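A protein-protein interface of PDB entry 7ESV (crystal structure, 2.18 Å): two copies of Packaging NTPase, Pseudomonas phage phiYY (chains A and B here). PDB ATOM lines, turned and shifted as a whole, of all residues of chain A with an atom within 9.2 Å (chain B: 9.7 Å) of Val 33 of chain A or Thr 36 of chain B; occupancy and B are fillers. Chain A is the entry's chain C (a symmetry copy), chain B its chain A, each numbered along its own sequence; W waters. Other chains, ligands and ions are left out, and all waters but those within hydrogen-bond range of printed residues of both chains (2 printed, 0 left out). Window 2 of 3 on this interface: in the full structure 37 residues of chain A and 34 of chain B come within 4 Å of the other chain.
Of the printed residues of chain B, Ala 30 of chain A touches Glu 38.
Printed residues of chain B within 4 Å of Val 33 of chain A: Thr 36, Thr 37 and Glu 38.
No residue of chain B comes within 4 Å of Gly 48 of chain A.
Glu 34 of chain B touches none of the printed residues of chain A.
Printed residues of chain A within 4 Å of Thr 36 of chain B: Val 32 and Val 33.
Printed residues of chain A within 4 Å of Glu 38 of chain B: Val 29, Ala 30, Leu 31, Val 32 and Val 33.
The nearest residue of chain B that does not touch Val 33 of chain A is Ala 39 of chain B (6.5 Å).
The nearest printed residue of chain B that does not touch Val 29 of chain A is Lys 42 of chain B (5.5 Å).
Hydrophobic or aromatic side chains of chain A that line the printed part of chain B: Ala 30, Leu 31, Val 32, Val 33 and Val 105.
Hydrophobic or aromatic side chains of chain B that line the printed part of chain A: Ala 41 and Leu 50.
Among the printed residues, 15 pairs touch across the chains.
Among the printed residues, no Asp or Glu carboxylate lies within 4 Å of a Lys or Arg side-chain nitrogen of the other chain.
Val 32 of chain A touches Ala 35 of chain B, but with the chains exchanged Ala 35 of chain A does not touch Val 32 of chain B (20.4 Å).
Val 32 of chain A touches Thr 36 of chain B, but with the chains exchanged Thr 36 of chain A does not touch Val 32 of chain B (20.2 Å).
Of the 15 pairs that touch across the chains among the printed residues, none has its exchanged pair printed and touching as well.
The backbone NH of Thr 37 of chain B sits at hydrogen-bond distance from the side-chain carboxylate of Glu 40 of chain B, 3.2 Å away.
O of Ala 41 of chain B is in hydrogen-bond range of N of Leu 50 of chain B, 2.8 Å away.
O of Gly 48 of chain B lies within hydrogen-bond range of N of Ala 35 of chain B.
The backbone NH of Ala 30 of chain A sits at hydrogen-bond distance from the backbone carbonyl oxygen of Arg 46 of chain A, at 2.9 Å.
Water W1 bridges the backbone carbonyl oxygen (O) of Leu 31 of chain A and the guanidinium group (NH1) of Arg 111 of chain B.
Water W2 lies within hydrogen-bond range of NH2 of Arg 111 of chain B and O of Ala 30 of chain A.
The guanidinium group (NE) of Arg 111 of chain B is in hydrogen-bond range of the backbone carbonyl oxygen (O) of Pro 104 of chain A (3.3 Å).
The backbone NH (N) of Val 33 of chain A is in hydrogen-bond range of the side-chain carboxylate (OE1) of Glu 38 of chain B (2.9 Å).
The guanidinium group (NH2) of Arg 111 of chain B lies within hydrogen-bond range of the backbone carbonyl oxygen (O) of Leu 31 of chain A.
The side-chain carboxylate (OE2) of Glu 38 of chain B is in hydrogen-bond range of the backbone NH (N) of Leu 31 of chain A, at 2.8 Å.
OE1 of Glu 38 of chain B is in hydrogen-bond range of N of Val 32 of chain A, 3.0 Å away.
Among the printed residues, merely in contact across the chains: Val 29 of chain A with Glu 38 of chain B (3.7 Å), Ala 30 of chain A with Glu 38 of chain B (3.4 Å), Leu 31 of chain A with Ala 41 of chain B (3.98 Å), Leu 31 of chain A with Leu 50 of chain B (3.8 Å), Val 32 of chain A with Ala 35 of chain B (3.5 Å), Val 32 of chain A with Thr 36 of chain B (3.7 Å), Val 32 of chain A with Thr 37 of chain B (3.4 Å), Val 33 of chain A with Thr 36 of chain B (3.8 Å), Val 33 of chain A with Thr 37 of chain B (3.97 Å) and Val 105 of chain A with Arg 111 of chain B (3.6 Å).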
ATOM      1  N   THR A  28      -7.999 -10.585 -23.776  1.00  0.00           N
ATOM      2  CA  THR A  28      -7.837 -11.548 -24.857  1.00  0.00           C
ATOM      3  C   THR A  28      -6.593 -11.322 -25.702  1.00  0.00           C
ATOM      4  O   THR A  28      -6.395 -12.042 -26.686  1.00  0.00           O
ATOM      5  CB  THR A  28      -9.073 -11.529 -25.763  1.00  0.00           C
ATOM      6  OG1 THR A  28      -9.405 -10.175 -26.095  1.00  0.00           O
ATOM      7  CG2 THR A  28     -10.256 -12.182 -25.063  1.00  0.00           C
ATOM      8  N   VAL A  29      -5.752 -10.348 -25.360  1.00  0.00           N
ATOM      9  CA  VAL A  29      -4.520 -10.144 -26.114  1.00  0.00           C
ATOM     10  C   VAL A  29      -3.551 -11.272 -25.784  1.00  0.00           C
ATOM     11  O   VAL A  29      -3.203 -11.489 -24.618  1.00  0.00           O
ATOM     12  CB  VAL A  29      -3.902  -8.775 -25.807  1.00  0.00           C
ATOM     13  CG1 VAL A  29      -2.561  -8.631 -26.520  1.00  0.00           C
ATOM     14  CG2 VAL A  29      -4.849  -7.659 -26.215  1.00  0.00           C
ATOM     15  N   ALA A  30      -3.121 -12.005 -26.809  1.00  0.00           N
ATOM     16  CA  ALA A  30      -2.122 -13.044 -26.611  1.00  0.00           C
ATOM     17  C   ALA A  30      -0.804 -12.419 -26.171  1.00  0.00           C
ATOM     18  O   ALA A  30      -0.269 -11.531 -26.842  1.00  0.00           O
ATOM     19  CB  ALA A  30      -1.931 -13.847 -27.896  1.00  0.00           C
ATOM     20  N   LEU A  31      -0.282 -12.879 -25.032  1.00  0.00           N
ATOM     21  CA  LEU A  31       0.921 -12.289 -24.459  1.00  0.00           C
ATOM     22  C   LEU A  31       2.179 -13.128 -24.638  1.00  0.00           C
ATOM     23  O   LEU A  31       3.281 -12.582 -24.498  1.00  0.00           O
ATOM     24  CB  LEU A  31       0.728 -12.010 -22.961  1.00  0.00           C
ATOM     25  CG  LEU A  31      -0.498 -11.218 -22.503  1.00  0.00           C
ATOM     26  CD1 LEU A  31      -0.461 -10.993 -20.998  1.00  0.00           C
ATOM     27  CD2 LEU A  31      -0.581  -9.888 -23.239  1.00  0.00           C
ATOM     28  N   VAL A  32       2.061 -14.423 -24.946  1.00  0.00           N
ATOM     29  CA  VAL A  32       3.249 -15.275 -24.969  1.00  0.00           C
ATOM     30  C   VAL A  32       3.145 -16.371 -26.029  1.00  0.00           C
ATOM     31  O   VAL A  32       4.171 -16.883 -26.498  1.00  0.00           O
ATOM     32  CB  VAL A  32       3.510 -15.876 -23.571  1.00  0.00           C
ATOM     33  CG1 VAL A  32       2.514 -16.985 -23.260  1.00  0.00           C
ATOM     34  CG2 VAL A  32       4.949 -16.366 -23.444  1.00  0.00           C
ATOM     35  N   VAL A  33       1.926 -16.736 -26.425  1.00  0.00           N
ATOM     36  CA  VAL A  33       1.721 -17.763 -27.442  1.00  0.00           C
ATOM     37  C   VAL A  33       1.539 -17.062 -28.782  1.00  0.00           C
ATOM     38  O   VAL A  33       0.558 -16.330 -28.984  1.00  0.00           O
ATOM     39  CB  VAL A  33       0.513 -18.653 -27.116  1.00  0.00           C
ATOM     40  CG1 VAL A  33       0.448 -19.840 -28.079  1.00  0.00           C
ATOM     41  CG2 VAL A  33       0.564 -19.124 -25.672  1.00  0.00           C
ATOM     42  N   GLU A  34       2.481 -17.278 -29.699  1.00  0.00           N
ATOM     43  CA  GLU A  34       2.391 -16.717 -31.036  1.00  0.00           C
ATOM     44  C   GLU A  34       2.211 -17.834 -32.052  1.00  0.00           C
ATOM     45  O   GLU A  34       2.452 -19.014 -31.774  1.00  0.00           O
ATOM     46  CB  GLU A  34       3.634 -15.886 -31.389  1.00  0.00           C
ATOM     47  CG  GLU A  34       4.930 -16.666 -31.454  1.00  0.00           C
ATOM     48  CD  GLU A  34       6.118 -15.759 -31.689  1.00  0.00           C
ATOM     49  OE1 GLU A  34       6.215 -15.185 -32.796  1.00  0.00           O
ATOM     50  OE2 GLU A  34       6.952 -15.618 -30.770  1.00  0.00           O
ATOM     51  N   ALA A  35       1.778 -17.431 -33.243  1.00  0.00           N
ATOM     52  CA  ALA A  35       1.515 -18.378 -34.312  1.00  0.00           C
ATOM     53  C   ALA A  35       2.750 -19.207 -34.637  1.00  0.00           C
ATOM     54  O   ALA A  35       3.864 -18.686 -34.720  1.00  0.00           O
ATOM     55  CB  ALA A  35       1.039 -17.629 -35.554  1.00  0.00           C
ATOM     56  N   THR A  36       2.541 -20.513 -34.801  1.00  0.00           N
ATOM     57  CA  THR A  36       3.594 -21.426 -35.210  1.00  0.00           C
ATOM     58  C   THR A  36       3.278 -22.150 -36.511  1.00  0.00           C
ATOM     59  O   THR A  36       4.146 -22.862 -37.031  1.00  0.00           O
ATOM     60  CB  THR A  36       3.873 -22.460 -34.103  1.00  0.00           C
ATOM     61  OG1 THR A  36       4.995 -23.271 -34.466  1.00  0.00           O
ATOM     62  CG2 THR A  36       2.661 -23.354 -33.880  1.00  0.00           C
ATOM     63  N   GLU A  40      -2.466 -20.465 -38.050  1.00  0.00           N
ATOM     64  CA  GLU A  40      -2.396 -19.549 -36.918  1.00  0.00           C
ATOM     65  C   GLU A  40      -1.855 -18.190 -37.345  1.00  0.00           C
ATOM     66  O   GLU A  40      -2.307 -17.150 -36.849  1.00  0.00           O
ATOM     67  CB  GLU A  40      -1.531 -20.152 -35.811  1.00  0.00           C
ATOM     68  CG  GLU A  40      -2.135 -21.383 -35.152  1.00  0.00           C
ATOM     69  CD  GLU A  40      -1.125 -22.163 -34.334  1.00  0.00           C
ATOM     70  OE1 GLU A  40      -1.471 -23.262 -33.851  1.00  0.00           O
ATOM     71  OE2 GLU A  40       0.013 -21.676 -34.172  1.00  0.00           O
ATOM     72  N   LYS A  43      -4.331 -15.366 -38.309  1.00  0.00           N
ATOM     73  CA  LYS A  43      -5.194 -14.743 -37.316  1.00  0.00           C
ATOM     74  C   LYS A  43      -4.797 -13.287 -37.076  1.00  0.00           C
ATOM     75  O   LYS A  43      -3.763 -12.802 -37.546  1.00  0.00           O
ATOM     76  CB  LYS A  43      -5.158 -15.522 -36.005  1.00  0.00           C
ATOM     77  CG  LYS A  43      -5.448 -17.011 -36.115  1.00  0.00           C
ATOM     78  CD  LYS A  43      -5.480 -17.640 -34.727  1.00  0.00           C
ATOM     79  CE  LYS A  43      -6.588 -18.673 -34.597  1.00  0.00           C
ATOM     80  NZ  LYS A  43      -6.629 -19.263 -33.229  1.00  0.00           N
ATOM     81  N   SER A  44      -5.636 -12.588 -36.314  1.00  0.00           N
ATOM     82  CA  SER A  44      -5.383 -11.201 -35.953  1.00  0.00           C
ATOM     83  C   SER A  44      -4.156 -11.089 -35.053  1.00  0.00           C
ATOM     84  O   SER A  44      -3.702 -12.064 -34.446  1.00  0.00           O
ATOM     85  CB  SER A  44      -6.602 -10.606 -35.246  1.00  0.00           C
ATOM     86  OG  SER A  44      -6.740 -11.137 -33.939  1.00  0.00           O
ATOM     87  N   LEU A  45      -3.622  -9.869 -34.967  1.00  0.00           N
ATOM     88  CA  LEU A  45      -2.485  -9.625 -34.085  1.00  0.00           C
ATOM     89  C   LEU A  45      -2.869  -9.824 -32.626  1.00  0.00           C
ATOM     90  O   LEU A  45      -2.045 -10.261 -31.813  1.00  0.00           O
ATOM     91  CB  LEU A  45      -1.940  -8.216 -34.309  1.00  0.00           C
ATOM     92  CG  LEU A  45      -1.669  -7.844 -35.764  1.00  0.00           C
ATOM     93  CD1 LEU A  45      -1.261  -6.391 -35.851  1.00  0.00           C
ATOM     94  CD2 LEU A  45      -0.598  -8.744 -36.363  1.00  0.00           C
ATOM     95  N   ARG A  46      -4.115  -9.496 -32.272  1.00  0.00           N
ATOM     96  CA  ARG A  46      -4.619  -9.797 -30.937  1.00  0.00           C
ATOM     97  C   ARG A  46      -4.445 -11.272 -30.598  1.00  0.00           C
ATOM     98  O   ARG A  46      -4.091 -11.624 -29.467  1.00  0.00           O
ATOM     99  CB  ARG A  46      -6.094  -9.405 -30.833  1.00  0.00           C
ATOM    100  CG  ARG A  46      -6.824 -10.054 -29.666  1.00  0.00           C
ATOM    101  CD  ARG A  46      -8.230  -9.508 -29.509  1.00  0.00           C
ATOM    102  NE  ARG A  46      -8.265  -8.054 -29.611  1.00  0.00           N
ATOM    103  CZ  ARG A  46      -8.233  -7.236 -28.565  1.00  0.00           C
ATOM    104  NH1 ARG A  46      -8.166  -7.730 -27.336  1.00  0.00           N
ATOM    105  NH2 ARG A  46      -8.269  -5.923 -28.746  1.00  0.00           N
ATOM    106  N   GLU A  47      -4.673 -12.148 -31.571  1.00  0.00           N
ATOM    107  CA  GLU A  47      -4.657 -13.586 -31.350  1.00  0.00           C
ATOM    108  C   GLU A  47      -3.276 -14.208 -31.508  1.00  0.00           C
ATOM    109  O   GLU A  47      -3.154 -15.434 -31.430  1.00  0.00           O
ATOM    110  CB  GLU A  47      -5.644 -14.268 -32.303  1.00  0.00           C
ATOM    111  CG  GLU A  47      -7.074 -14.257 -31.795  1.00  0.00           C
ATOM    112  CD  GLU A  47      -8.094 -14.060 -32.900  1.00  0.00           C
ATOM    113  OE1 GLU A  47      -7.764 -14.310 -34.078  1.00  0.00           O
ATOM    114  OE2 GLU A  47      -9.232 -13.651 -32.586  1.00  0.00           O
ATOM    115  N   GLY A  48      -2.237 -13.406 -31.717  1.00  0.00           N
ATOM    116  CA  GLY A  48      -0.912 -13.938 -31.942  1.00  0.00           C
ATOM    117  C   GLY A  48      -0.586 -14.250 -33.383  1.00  0.00           C
ATOM    118  O   GLY A  48       0.450 -14.872 -33.646  1.00  0.00           O
ATOM    119  N   GLY A  49      -1.440 -13.851 -34.325  1.00  0.00           N
ATOM    120  CA  GLY A  49      -1.155 -14.010 -35.732  1.00  0.00           C
ATOM    121  C   GLY A  49      -0.321 -12.864 -36.272  1.00  0.00           C
ATOM    122  O   GLY A  49       0.117 -11.971 -35.547  1.00  0.00           O
ATOM    123  N   PRO A 104       1.623  -6.592 -30.201  1.00  0.00           N
ATOM    124  CA  PRO A 104       1.356  -7.990 -30.564  1.00  0.00           C
ATOM    125  C   PRO A 104       2.568  -8.881 -30.325  1.00  0.00           C
ATOM    126  O   PRO A 104       3.714  -8.429 -30.341  1.00  0.00           O
ATOM    127  CB  PRO A 104       0.998  -7.917 -32.054  1.00  0.00           C
ATOM    128  CG  PRO A 104       0.710  -6.477 -32.336  1.00  0.00           C
ATOM    129  CD  PRO A 104       1.471  -5.670 -31.339  1.00  0.00           C
ATOM    130  N   VAL A 105       2.296 -10.165 -30.105  1.00  0.00           N
ATOM    131  CA  VAL A 105       3.337 -11.086 -29.662  1.00  0.00           C
ATOM    132  C   VAL A 105       4.125 -11.685 -30.827  1.00  0.00           C
ATOM    133  O   VAL A 105       5.293 -12.050 -30.655  1.00  0.00           O
ATOM    134  CB  VAL A 105       2.720 -12.192 -28.784  1.00  0.00           C
ATOM    135  CG1 VAL A 105       1.849 -13.125 -29.617  1.00  0.00           C
ATOM    136  CG2 VAL A 105       3.807 -12.969 -28.052  1.00  0.00           C
ATOM    137  N   ALA A 106       3.521 -11.785 -32.010  1.00  0.00           N
ATOM    138  CA  ALA A 106       4.173 -12.446 -33.135  1.00  0.00           C
ATOM    139  C   ALA A 106       5.441 -11.703 -33.537  1.00  0.00           C
ATOM    140  O   ALA A 106       5.417 -10.493 -33.782  1.00  0.00           O
ATOM    141  CB  ALA A 106       3.211 -12.541 -34.317  1.00  0.00           C
ATOM    142  N   LYS A 107       6.550 -12.439 -33.614  1.00  0.00           N
ATOM    143  CA  LYS A 107       7.858 -11.828 -33.814  1.00  0.00           C
ATOM    144  C   LYS A 107       8.161 -11.515 -35.274  1.00  0.00           C
ATOM    145  O   LYS A 107       9.053 -10.704 -35.543  1.00  0.00           O
ATOM    146  CB  LYS A 107       8.943 -12.742 -33.238  1.00  0.00           C
ATOM    147  CG  LYS A 107       8.764 -12.995 -31.750  1.00  0.00           C
ATOM    148  CD  LYS A 107       9.734 -14.025 -31.198  1.00  0.00           C
ATOM    149  CE  LYS A 107       9.786 -13.927 -29.679  1.00  0.00           C
ATOM    150  NZ  LYS A 107      10.096 -15.226 -29.022  1.00  0.00           N
ATOM    151  N   VAL B  32      13.568 -18.942 -12.820  1.00  0.00           N
ATOM    152  CA  VAL B  32      13.938 -19.496 -14.120  1.00  0.00           C
ATOM    153  C   VAL B  32      12.701 -19.852 -14.933  1.00  0.00           C
ATOM    154  O   VAL B  32      12.713 -19.769 -16.167  1.00  0.00           O
ATOM    155  CB  VAL B  32      14.860 -20.723 -13.968  1.00  0.00           C
ATOM    156  CG1 VAL B  32      16.108 -20.358 -13.199  1.00  0.00           C
ATOM    157  CG2 VAL B  32      14.135 -21.869 -13.276  1.00  0.00           C
ATOM    158  N   VAL B  33      11.629 -20.252 -14.260  1.00  0.00           N
ATOM    159  CA  VAL B  33      10.421 -20.714 -14.933  1.00  0.00           C
ATOM    160  C   VAL B  33       9.511 -19.511 -15.150  1.00  0.00           C
ATOM    161  O   VAL B  33       9.011 -18.913 -14.194  1.00  0.00           O
ATOM    162  CB  VAL B  33       9.712 -21.816 -14.139  1.00  0.00           C
ATOM    163  CG1 VAL B  33       8.498 -22.313 -14.911  1.00  0.00           C
ATOM    164  CG2 VAL B  33      10.670 -22.960 -13.854  1.00  0.00           C
ATOM    165  N   GLU B  34       9.307 -19.158 -16.412  1.00  0.00           N
ATOM    166  CA  GLU B  34       8.422 -18.078 -16.809  1.00  0.00           C
ATOM    167  C   GLU B  34       7.228 -18.648 -17.560  1.00  0.00           C
ATOM    168  O   GLU B  34       7.231 -19.804 -17.991  1.00  0.00           O
ATOM    169  CB  GLU B  34       9.156 -17.067 -17.692  1.00  0.00           C
ATOM    170  CG  GLU B  34       9.733 -17.691 -18.949  1.00  0.00           C
ATOM    171  CD  GLU B  34      10.352 -16.671 -19.878  1.00  0.00           C
ATOM    172  OE1 GLU B  34       9.708 -15.633 -20.138  1.00  0.00           O
ATOM    173  OE2 GLU B  34      11.482 -16.909 -20.351  1.00  0.00           O
ATOM    174  N   ALA B  35       6.210 -17.808 -17.719  1.00  0.00           N
ATOM    175  CA  ALA B  35       4.996 -18.214 -18.411  1.00  0.00           C
ATOM    176  C   ALA B  35       5.303 -18.682 -19.827  1.00  0.00           C
ATOM    177  O   ALA B  35       6.071 -18.046 -20.554  1.00  0.00           O
ATOM    178  CB  ALA B  35       4.011 -17.046 -18.449  1.00  0.00           C
ATOM    179  N   THR B  36       4.710 -19.815 -20.206  1.00  0.00           N
ATOM    180  CA  THR B  36       4.737 -20.286 -21.581  1.00  0.00           C
ATOM    181  C   THR B  36       3.351 -20.391 -22.199  1.00  0.00           C
ATOM    182  O   THR B  36       3.249 -20.604 -23.412  1.00  0.00           O
ATOM    183  CB  THR B  36       5.429 -21.656 -21.681  1.00  0.00           C
ATOM    184  OG1 THR B  36       4.772 -22.594 -20.820  1.00  0.00           O
ATOM    185  CG2 THR B  36       6.897 -21.545 -21.288  1.00  0.00           C
ATOM    186  N   THR B  37       2.289 -20.253 -21.406  1.00  0.00           N
ATOM    187  CA  THR B  37       0.923 -20.293 -21.898  1.00  0.00           C
ATOM    188  C   THR B  37       0.224 -18.993 -21.525  1.00  0.00           C
ATOM    189  O   THR B  37       0.686 -18.244 -20.660  1.00  0.00           O
ATOM    190  CB  THR B  37       0.145 -21.491 -21.327  1.00  0.00           C
ATOM    191  OG1 THR B  37      -0.078 -21.294 -19.926  1.00  0.00           O
ATOM    192  CG2 THR B  37       0.928 -22.779 -21.526  1.00  0.00           C
ATOM    193  N   GLU B  38      -0.904 -18.732 -22.192  1.00  0.00           N
ATOM    194  CA  GLU B  38      -1.671 -17.524 -21.900  1.00  0.00           C
ATOM    195  C   GLU B  38      -2.157 -17.516 -20.456  1.00  0.00           C
ATOM    196  O   GLU B  38      -2.246 -16.453 -19.828  1.00  0.00           O
ATOM    197  CB  GLU B  38      -2.853 -17.403 -22.862  1.00  0.00           C
ATOM    198  CG  GLU B  38      -2.490 -16.983 -24.283  1.00  0.00           C
ATOM    199  CD  GLU B  38      -1.523 -15.811 -24.335  1.00  0.00           C
ATOM    200  OE1 GLU B  38      -0.478 -15.929 -25.008  1.00  0.00           O
ATOM    201  OE2 GLU B  38      -1.812 -14.768 -23.710  1.00  0.00           O
ATOM    202  N   ALA B  39      -2.478 -18.692 -19.913  1.00  0.00           N
ATOM    203  CA  ALA B  39      -2.928 -18.778 -18.527  1.00  0.00           C
ATOM    204  C   ALA B  39      -1.836 -18.321 -17.568  1.00  0.00           C
ATOM    205  O   ALA B  39      -2.086 -17.527 -16.654  1.00  0.00           O
ATOM    206  CB  ALA B  39      -3.365 -20.208 -18.205  1.00  0.00           C
ATOM    207  N   GLU B  40      -0.614 -18.816 -17.763  1.00  0.00           N
ATOM    208  CA  GLU B  40       0.483 -18.430 -16.885  1.00  0.00           C
ATOM    209  C   GLU B  40       0.900 -16.980 -17.111  1.00  0.00           C
ATOM    210  O   GLU B  40       1.423 -16.339 -16.193  1.00  0.00           O
ATOM    211  CB  GLU B  40       1.667 -19.377 -17.088  1.00  0.00           C
ATOM    212  CG  GLU B  40       1.279 -20.849 -17.074  1.00  0.00           C
ATOM    213  CD  GLU B  40       2.419 -21.765 -17.473  1.00  0.00           C
ATOM    214  OE1 GLU B  40       3.061 -21.502 -18.513  1.00  0.00           O
ATOM    215  OE2 GLU B  40       2.670 -22.753 -16.753  1.00  0.00           O
ATOM    216  N   ALA B  41       0.669 -16.446 -18.315  1.00  0.00           N
ATOM    217  CA  ALA B  41       1.039 -15.062 -18.598  1.00  0.00           C
ATOM    218  C   ALA B  41       0.221 -14.082 -17.773  1.00  0.00           C
ATOM    219  O   ALA B  41       0.700 -12.988 -17.448  1.00  0.00           O
ATOM    220  CB  ALA B  41       0.872 -14.767 -20.088  1.00  0.00           C
ATOM    221  N   LYS B  42      -1.009 -14.452 -17.421  1.00  0.00           N
ATOM    222  CA  LYS B  42      -1.859 -13.584 -16.618  1.00  0.00           C
ATOM    223  C   LYS B  42      -1.426 -13.497 -15.158  1.00  0.00           C
ATOM    224  O   LYS B  42      -1.931 -12.628 -14.440  1.00  0.00           O
ATOM    225  CB  LYS B  42      -3.310 -14.060 -16.692  1.00  0.00           C
ATOM    226  CG  LYS B  42      -3.841 -14.207 -18.109  1.00  0.00           C
ATOM    227  CD  LYS B  42      -5.352 -14.100 -18.152  1.00  0.00           C
ATOM    228  CE  LYS B  42      -5.880 -14.451 -19.530  1.00  0.00           C
ATOM    229  NZ  LYS B  42      -6.190 -13.224 -20.314  1.00  0.00           N
ATOM    230  N   LYS B  43      -0.520 -14.358 -14.697  1.00  0.00           N
ATOM    231  CA  LYS B  43      -0.109 -14.319 -13.301  1.00  0.00           C
ATOM    232  C   LYS B  43       0.814 -13.133 -13.043  1.00  0.00           C
ATOM    233  O   LYS B  43       1.244 -12.424 -13.956  1.00  0.00           O
ATOM    234  CB  LYS B  43       0.600 -15.610 -12.891  1.00  0.00           C
ATOM    235  CG  LYS B  43      -0.263 -16.833 -12.861  1.00  0.00           C
ATOM    236  CD  LYS B  43       0.426 -18.056 -12.281  1.00  0.00           C
ATOM    237  CE  LYS B  43       1.434 -18.597 -13.264  1.00  0.00           C
ATOM    238  NZ  LYS B  43       1.893 -19.934 -12.801  1.00  0.00           N
ATOM    239  N   GLU B  47       5.314 -14.521  -9.871  1.00  0.00           N
ATOM    240  CA  GLU B  47       5.037 -15.888 -10.296  1.00  0.00           C
ATOM    241  C   GLU B  47       5.541 -16.205 -11.698  1.00  0.00           C
ATOM    242  O   GLU B  47       5.281 -17.307 -12.190  1.00  0.00           O
ATOM    243  CB  GLU B  47       3.533 -16.164 -10.239  1.00  0.00           C
ATOM    244  CG  GLU B  47       2.959 -16.244  -8.840  1.00  0.00           C
ATOM    245  CD  GLU B  47       1.457 -16.047  -8.825  1.00  0.00           C
ATOM    246  OE1 GLU B  47       0.993 -14.969  -9.254  1.00  0.00           O
ATOM    247  OE2 GLU B  47       0.741 -16.974  -8.394  1.00  0.00           O
ATOM    248  N   GLY B  48       6.242 -15.287 -12.352  1.00  0.00           N
ATOM    249  CA  GLY B  48       6.700 -15.521 -13.704  1.00  0.00           C
ATOM    250  C   GLY B  48       5.706 -15.172 -14.786  1.00  0.00           C
ATOM    251  O   GLY B  48       5.910 -15.566 -15.941  1.00  0.00           O
ATOM    252  N   GLY B  49       4.633 -14.461 -14.452  1.00  0.00           N
ATOM    253  CA  GLY B  49       3.706 -13.964 -15.442  1.00  0.00           C
ATOM    254  C   GLY B  49       4.181 -12.653 -16.039  1.00  0.00           C
ATOM    255  O   GLY B  49       5.300 -12.191 -15.811  1.00  0.00           O
ATOM    256  N   LEU B  50       3.293 -12.042 -16.819  1.00  0.00           N
ATOM    257  CA  LEU B  50       3.601 -10.808 -17.525  1.00  0.00           C
ATOM    258  C   LEU B  50       2.675  -9.661 -17.152  1.00  0.00           C
ATOM    259  O   LEU B  50       2.782  -8.580 -17.744  1.00  0.00           O
ATOM    260  CB  LEU B  50       3.543 -11.038 -19.043  1.00  0.00           C
ATOM    261  CG  LEU B  50       4.707 -11.794 -19.689  1.00  0.00           C
ATOM    262  CD1 LEU B  50       4.577 -13.294 -19.475  1.00  0.00           C
ATOM    263  CD2 LEU B  50       4.766 -11.477 -21.172  1.00  0.00           C
ATOM    264  N   VAL B 105      11.165 -12.671 -14.083  1.00  0.00           N
ATOM    265  CA  VAL B 105      11.812 -13.619 -14.985  1.00  0.00           C
ATOM    266  C   VAL B 105      11.233 -13.614 -16.398  1.00  0.00           C
ATOM    267  O   VAL B 105      11.948 -13.970 -17.348  1.00  0.00           O
ATOM    268  CB  VAL B 105      11.743 -15.039 -14.390  1.00  0.00           C
ATOM    269  CG1 VAL B 105      10.314 -15.565 -14.394  1.00  0.00           C
ATOM    270  CG2 VAL B 105      12.683 -15.990 -15.126  1.00  0.00           C
ATOM    271  N   ALA B 106       9.973 -13.211 -16.568  1.00  0.00           N
ATOM    272  CA  ALA B 106       9.319 -13.296 -17.868  1.00  0.00           C
ATOM    273  C   ALA B 106       9.988 -12.357 -18.857  1.00  0.00           C
ATOM    274  O   ALA B 106      10.134 -11.159 -18.598  1.00  0.00           O
ATOM    275  CB  ALA B 106       7.840 -12.958 -17.746  1.00  0.00           C
ATOM    276  N   LYS B 107      10.381 -12.895 -20.002  1.00  0.00           N
ATOM    277  CA  LYS B 107      11.267 -12.123 -20.857  1.00  0.00           C
ATOM    278  C   LYS B 107      10.532 -11.162 -21.793  1.00  0.00           C
ATOM    279  O   LYS B 107      11.160 -10.268 -22.373  1.00  0.00           O
ATOM    280  CB  LYS B 107      12.139 -13.084 -21.653  1.00  0.00           C
ATOM    281  CG  LYS B 107      12.966 -13.974 -20.804  1.00  0.00           C
ATOM    282  CD  LYS B 107      13.952 -13.231 -19.964  1.00  0.00           C
ATOM    283  CE  LYS B 107      14.929 -14.203 -19.332  1.00  0.00           C
ATOM    284  NZ  LYS B 107      14.281 -15.120 -18.205  1.00  0.00           N
ATOM    285  N   ARG B 111       8.674  -5.973 -24.457  1.00  0.00           N
ATOM    286  CA  ARG B 111       7.721  -5.820 -25.552  1.00  0.00           C
ATOM    287  C   ARG B 111       6.357  -5.365 -25.047  1.00  0.00           C
ATOM    288  O   ARG B 111       5.733  -4.481 -25.644  1.00  0.00           O
ATOM    289  CB  ARG B 111       7.594  -7.137 -26.316  1.00  0.00           C
ATOM    290  CG  ARG B 111       6.826  -7.030 -27.620  1.00  0.00           C
ATOM    291  CD  ARG B 111       6.331  -8.393 -28.079  1.00  0.00           C
ATOM    292  NE  ARG B 111       5.092  -8.790 -27.414  1.00  0.00           N
ATOM    293  CZ  ARG B 111       5.003  -9.762 -26.513  1.00  0.00           C
ATOM    294  NH1 ARG B 111       6.084 -10.447 -26.161  1.00  0.00           N
ATOM    295  NH2 ARG B 111       3.832 -10.056 -25.965  1.00  0.00           N
ATOM    296  N   VAL B 112       5.884  -5.949 -23.944  1.00  0.00           N
ATOM    297  CA  VAL B 112       4.499  -5.739 -23.534  1.00  0.00           C
ATOM    298  C   VAL B 112       4.291  -4.330 -22.985  1.00  0.00           C
ATOM    299  O   VAL B 112       3.191  -3.773 -23.087  1.00  0.00           O
ATOM    300  CB  VAL B 112       4.093  -6.828 -22.519  1.00  0.00           C
ATOM    301  CG1 VAL B 112       2.802  -6.466 -21.801  1.00  0.00           C
ATOM    302  CG2 VAL B 112       3.948  -8.165 -23.225  1.00  0.00           C
HETATM  303  O   HOH W   1       5.718 -12.894 -24.306  1.00  0.00           O
HETATM  304  O   HOH W   2       1.304  -9.162 -26.421  1.00  0.00           O
